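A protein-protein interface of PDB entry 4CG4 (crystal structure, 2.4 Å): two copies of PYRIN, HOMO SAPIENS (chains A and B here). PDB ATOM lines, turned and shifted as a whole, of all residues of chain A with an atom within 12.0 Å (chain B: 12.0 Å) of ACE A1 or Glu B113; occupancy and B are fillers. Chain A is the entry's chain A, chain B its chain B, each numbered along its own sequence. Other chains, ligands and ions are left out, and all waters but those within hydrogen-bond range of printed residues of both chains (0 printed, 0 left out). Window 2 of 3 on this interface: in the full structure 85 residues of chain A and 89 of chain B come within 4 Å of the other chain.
No position is printed for both chains. Of the 9 pairs that touch across the chains among the printed residues, none has its exchanged pair printed and touching as well.
N of Ser A2 lies within hydrogen-bond range of OE2 of Glu B113, 2.6 Å away.
O of Val A4 lies within hydrogen-bond range of ND1 of His A8, at 2.7 Å.
ACE A1 touches just one residue of chain B: Glu B113. No residue of chain B comes within 4 Å of Glu A3. Printed residues of chain B within 4 Å of Val A4: Leu B117 (3.7 Å). Ala A5 touches two residues of chain B. Of the printed residues of chain B, His A8 touches Leu B116 (3.96 Å), Leu B117 (3.8 Å) and Ile B120 (3.6 Å). Of the printed residues of chain B, Ile A12 touches Leu B116 (3.99 Å). No residue of chain A comes within 4 Å of Ser B112. Glu B113 touches just these residues of chain A: ACE A1, Ser A2 and Ala A5. No residue of chain A comes within 4 Å of Glu B115. Printed residues of chain A within 4 Å of Ile B120: His A8 (3.6 Å). The nearest residue of chain A that does not touch Glu B113 is Lys A9 (5.3 Å).
C of ACE A1 touches OE2 of Glu B113, at 3.6 Å. Leu B117 touches Val A4 (CD2 to CG2, 3.7 Å). Ala A5 touches Glu B113 (CB to OE2, 3.4 Å). N of Ala A5 touches CD2 of Leu B117, at 3.7 Å. His A8 touches Leu B116 (CB to CD2, 3.96 Å). CD2 of Leu B117 touches CE1 of His A8, at 3.8 Å. CD2 of His A8 touches CG1 of Ile B120, 3.6 Å away. CD1 of Ile A12 touches CD1 of Leu B116, 3.99 Å away.
Printed residues of chain A that touch a printed residue of chain B: ACE A1, Ser A2, Val A4, Ala A5, His A8 and Ile A12. Of the 15 printed residues of chain B, 4 touch a printed residue of chain A. Printed residues of chain B that touch a printed residue of chain A: Glu B113, Leu B116, Leu B117 and Ile B120. Among the printed residues, no Asp or Glu carboxylate lies within 4 Å of a Lys or Arg side-chain nitrogen of the other chain.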
ATOM      1  C   ACE A   1     -13.897  19.839 -19.254  1.00  0.00           C
ATOM      2  O   ACE A   1     -14.019  20.607 -18.282  1.00  0.00           O
ATOM      3  CH3 ACE A   1     -13.200  20.277 -20.519  1.00  0.00           C
ATOM      4  N   SER A   2     -14.458  18.567 -19.145  1.00  0.00           N
ATOM      5  CA  SER A   2     -14.443  17.549 -20.142  1.00  0.00           C
ATOM      6  C   SER A   2     -15.178  18.011 -21.382  1.00  0.00           C
ATOM      7  O   SER A   2     -16.040  18.868 -21.376  1.00  0.00           O
ATOM      8  CB  SER A   2     -15.126  16.218 -19.707  1.00  0.00           C
ATOM      9  OG  SER A   2     -16.293  16.460 -18.947  1.00  0.00           O
ATOM     10  N   GLU A   3     -14.837  17.385 -22.495  1.00  0.00           N
ATOM     11  CA  GLU A   3     -15.519  17.660 -23.727  1.00  0.00           C
ATOM     12  C   GLU A   3     -16.981  17.323 -23.673  1.00  0.00           C
ATOM     13  O   GLU A   3     -17.805  18.107 -24.133  1.00  0.00           O
ATOM     14  CB  GLU A   3     -14.880  16.906 -24.886  1.00  0.00           C
ATOM     15  CG  GLU A   3     -13.731  17.640 -25.506  1.00  0.00           C
ATOM     16  CD  GLU A   3     -14.204  18.845 -26.307  1.00  0.00           C
ATOM     17  OE1 GLU A   3     -15.253  18.740 -26.987  1.00  0.00           O
ATOM     18  OE2 GLU A   3     -13.547  19.907 -26.239  1.00  0.00           O
ATOM     19  N   VAL A   4     -17.328  16.190 -23.083  1.00  0.00           N
ATOM     20  CA  VAL A   4     -18.723  15.799 -23.076  1.00  0.00           C
ATOM     21  C   VAL A   4     -19.586  16.753 -22.279  1.00  0.00           C
ATOM     22  O   VAL A   4     -20.700  17.063 -22.680  1.00  0.00           O
ATOM     23  CB  VAL A   4     -18.952  14.410 -22.500  1.00  0.00           C
ATOM     24  CG1 VAL A   4     -18.830  13.398 -23.592  1.00  0.00           C
ATOM     25  CG2 VAL A   4     -18.040  14.148 -21.286  1.00  0.00           C
ATOM     26  N   ALA A   5     -19.041  17.243 -21.180  1.00  0.00           N
ATOM     27  CA  ALA A   5     -19.733  18.182 -20.319  1.00  0.00           C
ATOM     28  C   ALA A   5     -19.987  19.509 -21.035  1.00  0.00           C
ATOM     29  O   ALA A   5     -21.093  20.062 -20.981  1.00  0.00           O
ATOM     30  CB  ALA A   5     -18.917  18.400 -19.059  1.00  0.00           C
ATOM     31  N   LEU A   6     -18.956  20.019 -21.700  1.00  0.00           N
ATOM     32  CA  LEU A   6     -19.091  21.239 -22.473  1.00  0.00           C
ATOM     33  C   LEU A   6     -20.174  21.018 -23.503  1.00  0.00           C
ATOM     34  O   LEU A   6     -21.102  21.812 -23.609  1.00  0.00           O
ATOM     35  CB  LEU A   6     -17.774  21.640 -23.134  1.00  0.00           C
ATOM     36  CG  LEU A   6     -16.597  21.829 -22.162  1.00  0.00           C
ATOM     37  CD1 LEU A   6     -15.269  22.061 -22.898  1.00  0.00           C
ATOM     38  CD2 LEU A   6     -16.859  22.918 -21.127  1.00  0.00           C
ATOM     39  N   GLU A   7     -20.107  19.900 -24.217  1.00  0.00           N
ATOM     40  CA  GLU A   7     -21.170  19.606 -25.163  1.00  0.00           C
ATOM     41  C   GLU A   7     -22.557  19.593 -24.503  1.00  0.00           C
ATOM     42  O   GLU A   7     -23.508  20.165 -25.051  1.00  0.00           O
ATOM     43  CB  GLU A   7     -20.914  18.283 -25.872  1.00  0.00           C
ATOM     44  CG  GLU A   7     -19.874  18.421 -26.951  1.00  0.00           C
ATOM     45  CD  GLU A   7     -20.324  19.359 -28.063  1.00  0.00           C
ATOM     46  OE1 GLU A   7     -21.468  19.190 -28.542  1.00  0.00           O
ATOM     47  OE2 GLU A   7     -19.544  20.273 -28.435  1.00  0.00           O
ATOM     48  N   HIS A   8     -22.669  18.968 -23.335  1.00  0.00           N
ATOM     49  CA  HIS A   8     -23.937  18.900 -22.626  1.00  0.00           C
ATOM     50  C   HIS A   8     -24.472  20.320 -22.375  1.00  0.00           C
ATOM     51  O   HIS A   8     -25.628  20.623 -22.666  1.00  0.00           O
ATOM     52  CB  HIS A   8     -23.744  18.166 -21.308  1.00  0.00           C
ATOM     53  CG  HIS A   8     -23.891  16.673 -21.381  1.00  0.00           C
ATOM     54  ND1 HIS A   8     -22.999  15.862 -22.054  1.00  0.00           N
ATOM     55  CD2 HIS A   8     -24.711  15.834 -20.704  1.00  0.00           C
ATOM     56  CE1 HIS A   8     -23.335  14.597 -21.879  1.00  0.00           C
ATOM     57  NE2 HIS A   8     -24.366  14.552 -21.055  1.00  0.00           N
ATOM     58  N   LYS A   9     -23.582  21.188 -21.912  1.00  0.00           N
ATOM     59  CA  LYS A   9     -23.906  22.566 -21.613  1.00  0.00           C
ATOM     60  C   LYS A   9     -24.326  23.360 -22.856  1.00  0.00           C
ATOM     61  O   LYS A   9     -25.306  24.133 -22.814  1.00  0.00           O
ATOM     62  CB  LYS A   9     -22.705  23.215 -20.937  1.00  0.00           C
ATOM     63  CG  LYS A   9     -22.643  22.905 -19.468  1.00  0.00           C
ATOM     64  CD  LYS A   9     -21.466  23.577 -18.796  1.00  0.00           C
ATOM     65  CE  LYS A   9     -21.386  23.215 -17.310  1.00  0.00           C
ATOM     66  NZ  LYS A   9     -20.004  23.168 -16.755  1.00  0.00           N
ATOM     67  N   LYS A  10     -23.605  23.154 -23.959  1.00  0.00           N
ATOM     68  CA  LYS A  10     -23.992  23.756 -25.236  1.00  0.00           C
ATOM     69  C   LYS A  10     -25.401  23.357 -25.647  1.00  0.00           C
ATOM     70  O   LYS A  10     -26.284  24.225 -25.846  1.00  0.00           O
ATOM     71  CB  LYS A  10     -23.021  23.358 -26.335  1.00  0.00           C
ATOM     72  CG  LYS A  10     -21.732  24.100 -26.264  1.00  0.00           C
ATOM     73  CD  LYS A  10     -20.805  23.725 -27.392  1.00  0.00           C
ATOM     74  CE  LYS A  10     -19.466  24.442 -27.245  1.00  0.00           C
ATOM     75  NZ  LYS A  10     -18.448  23.955 -28.222  1.00  0.00           N
ATOM     76  N   ILE A  12     -27.681  22.219 -23.897  1.00  0.00           N
ATOM     77  CA  ILE A  12     -28.598  22.774 -22.920  1.00  0.00           C
ATOM     78  C   ILE A  12     -28.977  24.224 -23.243  1.00  0.00           C
ATOM     79  O   ILE A  12     -30.184  24.569 -23.324  1.00  0.00           O
ATOM     80  CB  ILE A  12     -27.997  22.685 -21.518  1.00  0.00           C
ATOM     81  CG1 ILE A  12     -28.157  21.268 -20.992  1.00  0.00           C
ATOM     82  CG2 ILE A  12     -28.725  23.597 -20.552  1.00  0.00           C
ATOM     83  CD1 ILE A  12     -27.369  20.976 -19.729  1.00  0.00           C
ATOM     84  N   ALA B 107     -32.505  23.876 -14.008  1.00  0.00           N
ATOM     85  CA  ALA B 107     -32.122  23.068 -12.877  1.00  0.00           C
ATOM     86  C   ALA B 107     -30.818  22.299 -13.151  1.00  0.00           C
ATOM     87  O   ALA B 107     -30.103  21.987 -12.204  1.00  0.00           O
ATOM     88  CB  ALA B 107     -33.231  22.123 -12.503  1.00  0.00           C
ATOM     89  N   LYS B 108     -30.544  21.890 -14.393  1.00  0.00           N
ATOM     90  CA  LYS B 108     -29.263  21.189 -14.634  1.00  0.00           C
ATOM     91  C   LYS B 108     -28.117  22.097 -14.187  1.00  0.00           C
ATOM     92  O   LYS B 108     -27.059  21.604 -13.776  1.00  0.00           O
ATOM     93  CB  LYS B 108     -29.041  20.748 -16.090  1.00  0.00           C
ATOM     94  CG  LYS B 108     -29.968  19.620 -16.546  1.00  0.00           C
ATOM     95  CD  LYS B 108     -30.155  18.539 -15.469  1.00  0.00           C
ATOM     96  CE  LYS B 108     -31.028  17.383 -15.962  1.00  0.00           C
ATOM     97  NZ  LYS B 108     -31.464  16.574 -14.775  1.00  0.00           N
ATOM     98  N   GLU B 109     -28.270  23.412 -14.330  1.00  0.00           N
ATOM     99  CA  GLU B 109     -27.238  24.277 -13.781  1.00  0.00           C
ATOM    100  C   GLU B 109     -27.288  24.080 -12.267  1.00  0.00           C
ATOM    101  O   GLU B 109     -28.238  23.520 -11.760  1.00  0.00           O
ATOM    102  CB  GLU B 109     -27.392  25.749 -14.178  1.00  0.00           C
ATOM    103  CG  GLU B 109     -26.169  26.559 -13.749  1.00  0.00           C
ATOM    104  CD  GLU B 109     -24.863  25.915 -14.282  1.00  0.00           C
ATOM    105  OE1 GLU B 109     -24.873  25.337 -15.400  1.00  0.00           O
ATOM    106  OE2 GLU B 109     -23.842  25.903 -13.553  1.00  0.00           O
ATOM    107  N   CYS B 110     -26.261  24.528 -11.562  1.00  0.00           N
ATOM    108  CA  CYS B 110     -26.125  24.347 -10.121  1.00  0.00           C
ATOM    109  C   CYS B 110     -25.717  22.890  -9.854  1.00  0.00           C
ATOM    110  O   CYS B 110     -25.627  22.473  -8.696  1.00  0.00           O
ATOM    111  CB  CYS B 110     -27.428  24.687  -9.359  1.00  0.00           C
ATOM    112  SG  CYS B 110     -28.061  26.430  -9.458  1.00  0.00           S
ATOM    113  N   GLN B 111     -25.470  22.120 -10.923  1.00  0.00           N
ATOM    114  CA  GLN B 111     -24.897  20.782 -10.768  1.00  0.00           C
ATOM    115  C   GLN B 111     -23.422  20.850 -11.042  1.00  0.00           C
ATOM    116  O   GLN B 111     -22.964  21.652 -11.848  1.00  0.00           O
ATOM    117  CB  GLN B 111     -25.523  19.746 -11.707  1.00  0.00           C
ATOM    118  CG  GLN B 111     -26.929  19.295 -11.343  1.00  0.00           C
ATOM    119  CD  GLN B 111     -27.466  18.210 -12.282  1.00  0.00           C
ATOM    120  OE1 GLN B 111     -27.011  18.062 -13.412  1.00  0.00           O
ATOM    121  NE2 GLN B 111     -28.407  17.423 -11.790  1.00  0.00           N
ATOM    122  N   SER B 112     -22.672  19.994 -10.377  1.00  0.00           N
ATOM    123  CA  SER B 112     -21.274  19.787 -10.731  1.00  0.00           C
ATOM    124  C   SER B 112     -21.195  19.066 -12.081  1.00  0.00           C
ATOM    125  O   SER B 112     -22.137  18.388 -12.485  1.00  0.00           O
ATOM    126  CB  SER B 112     -20.562  18.981  -9.641  1.00  0.00           C
ATOM    127  OG  SER B 112     -20.922  17.602  -9.713  1.00  0.00           O
ATOM    128  N   GLU B 113     -20.059  19.174 -12.755  1.00  0.00           N
ATOM    129  CA  GLU B 113     -19.843  18.484 -14.026  1.00  0.00           C
ATOM    130  C   GLU B 113     -20.193  16.985 -13.950  1.00  0.00           C
ATOM    131  O   GLU B 113     -20.960  16.433 -14.782  1.00  0.00           O
ATOM    132  CB  GLU B 113     -18.382  18.692 -14.430  1.00  0.00           C
ATOM    133  CG  GLU B 113     -17.953  18.020 -15.729  1.00  0.00           C
ATOM    134  CD  GLU B 113     -16.535  18.361 -16.125  1.00  0.00           C
ATOM    135  OE1 GLU B 113     -15.860  19.081 -15.356  1.00  0.00           O
ATOM    136  OE2 GLU B 113     -16.094  17.873 -17.188  1.00  0.00           O
ATOM    137  N   TRP B 114     -19.655  16.358 -12.907  1.00  0.00           N
ATOM    138  CA  TRP B 114     -19.826  14.933 -12.655  1.00  0.00           C
ATOM    139  C   TRP B 114     -21.299  14.654 -12.438  1.00  0.00           C
ATOM    140  O   TRP B 114     -21.837  13.701 -12.984  1.00  0.00           O
ATOM    141  CB  TRP B 114     -18.982  14.496 -11.444  1.00  0.00           C
ATOM    142  CG  TRP B 114     -18.860  13.014 -11.150  1.00  0.00           C
ATOM    143  CD1 TRP B 114     -19.061  12.415  -9.943  1.00  0.00           C
ATOM    144  CD2 TRP B 114     -18.505  11.968 -12.055  1.00  0.00           C
ATOM    145  NE1 TRP B 114     -18.843  11.065 -10.031  1.00  0.00           N
ATOM    146  CE2 TRP B 114     -18.501  10.760 -11.319  1.00  0.00           C
ATOM    147  CE3 TRP B 114     -18.188  11.927 -13.408  1.00  0.00           C
ATOM    148  CZ2 TRP B 114     -18.206   9.528 -11.896  1.00  0.00           C
ATOM    149  CZ3 TRP B 114     -17.874  10.703 -13.974  1.00  0.00           C
ATOM    150  CH2 TRP B 114     -17.891   9.520 -13.219  1.00  0.00           C
ATOM    151  N   GLU B 115     -21.958  15.473 -11.631  1.00  0.00           N
ATOM    152  CA  GLU B 115     -23.391  15.276 -11.432  1.00  0.00           C
ATOM    153  C   GLU B 115     -24.172  15.434 -12.738  1.00  0.00           C
ATOM    154  O   GLU B 115     -25.099  14.672 -13.008  1.00  0.00           O
ATOM    155  CB  GLU B 115     -23.930  16.243 -10.393  1.00  0.00           C
ATOM    156  CG  GLU B 115     -23.727  15.781  -8.976  1.00  0.00           C
ATOM    157  CD  GLU B 115     -24.115  16.834  -7.969  1.00  0.00           C
ATOM    158  OE1 GLU B 115     -24.652  17.905  -8.388  1.00  0.00           O
ATOM    159  OE2 GLU B 115     -23.882  16.573  -6.761  1.00  0.00           O
ATOM    160  N   LEU B 116     -23.781  16.428 -13.535  1.00  0.00           N
ATOM    161  CA  LEU B 116     -24.455  16.738 -14.797  1.00  0.00           C
ATOM    162  C   LEU B 116     -24.420  15.614 -15.788  1.00  0.00           C
ATOM    163  O   LEU B 116     -25.448  15.348 -16.429  1.00  0.00           O
ATOM    164  CB  LEU B 116     -23.846  17.974 -15.453  1.00  0.00           C
ATOM    165  CG  LEU B 116     -24.382  18.324 -16.839  1.00  0.00           C
ATOM    166  CD1 LEU B 116     -25.806  18.869 -16.721  1.00  0.00           C
ATOM    167  CD2 LEU B 116     -23.454  19.313 -17.531  1.00  0.00           C
ATOM    168  N   LEU B 117     -23.238  14.989 -15.946  1.00  0.00           N
ATOM    169  CA  LEU B 117     -23.061  13.950 -16.965  1.00  0.00           C
ATOM    170  C   LEU B 117     -23.936  12.736 -16.692  1.00  0.00           C
ATOM    171  O   LEU B 117     -24.452  12.097 -17.622  1.00  0.00           O
ATOM    172  CB  LEU B 117     -21.592  13.503 -17.023  1.00  0.00           C
ATOM    173  CG  LEU B 117     -20.604  14.553 -17.525  1.00  0.00           C
ATOM    174  CD1 LEU B 117     -19.189  14.096 -17.295  1.00  0.00           C
ATOM    175  CD2 LEU B 117     -20.855  14.901 -18.996  1.00  0.00           C
ATOM    176  N   GLN B 118     -24.101  12.453 -15.402  1.00  0.00           N
ATOM    177  CA  GLN B 118     -24.866  11.312 -14.901  1.00  0.00           C
ATOM    178  C   GLN B 118     -26.382  11.408 -14.931  1.00  0.00           C
ATOM    179  O   GLN B 118     -27.056  10.385 -15.024  1.00  0.00           O
ATOM    180  CB  GLN B 118     -24.443  10.991 -13.483  1.00  0.00           C
ATOM    181  CG  GLN B 118     -23.082  10.340 -13.431  1.00  0.00           C
ATOM    182  CD  GLN B 118     -22.775   9.860 -12.062  1.00  0.00           C
ATOM    183  OE1 GLN B 118     -22.046  10.511 -11.303  1.00  0.00           O
ATOM    184  NE2 GLN B 118     -23.357   8.717 -11.706  1.00  0.00           N
ATOM    185  N   ASP B 119     -26.922  12.622 -14.819  1.00  0.00           N
ATOM    186  CA  ASP B 119     -28.355  12.796 -14.600  1.00  0.00           C
ATOM    187  C   ASP B 119     -29.070  13.494 -15.751  1.00  0.00           C
ATOM    188  O   ASP B 119     -30.252  13.825 -15.650  1.00  0.00           O
ATOM    189  CB  ASP B 119     -28.602  13.574 -13.304  1.00  0.00           C
ATOM    190  CG  ASP B 119     -30.064  13.548 -12.879  1.00  0.00           C
ATOM    191  OD1 ASP B 119     -30.796  12.601 -13.251  1.00  0.00           O
ATOM    192  OD2 ASP B 119     -30.490  14.481 -12.174  1.00  0.00           O
ATOM    193  N   ILE B 120     -28.374  13.642 -16.867  1.00  0.00           N
ATOM    194  CA  ILE B 120     -28.874  14.420 -17.978  1.00  0.00           C
ATOM    195  C   ILE B 120     -30.204  13.859 -18.504  1.00  0.00           C
ATOM    196  O   ILE B 120     -31.065  14.623 -18.923  1.00  0.00           O
ATOM    197  CB  ILE B 120     -27.815  14.476 -19.116  1.00  0.00           C
ATOM    198  CG1 ILE B 120     -28.224  15.480 -20.204  1.00  0.00           C
ATOM    199  CG2 ILE B 120     -27.592  13.116 -19.740  1.00  0.00           C
ATOM    200  CD1 ILE B 120     -28.030  16.887 -19.822  1.00  0.00           C
ATOM    201  N   GLY B 121     -30.377  12.542 -18.460  1.00  0.00           N
ATOM    202  CA  GLY B 121     -31.572  11.868 -18.950  1.00  0.00           C
ATOM    203  C   GLY B 121     -31.955  12.237 -20.376  1.00  0.00           C
ATOM    204  O   GLY B 121     -31.098  12.577 -21.178  1.00  0.00           O
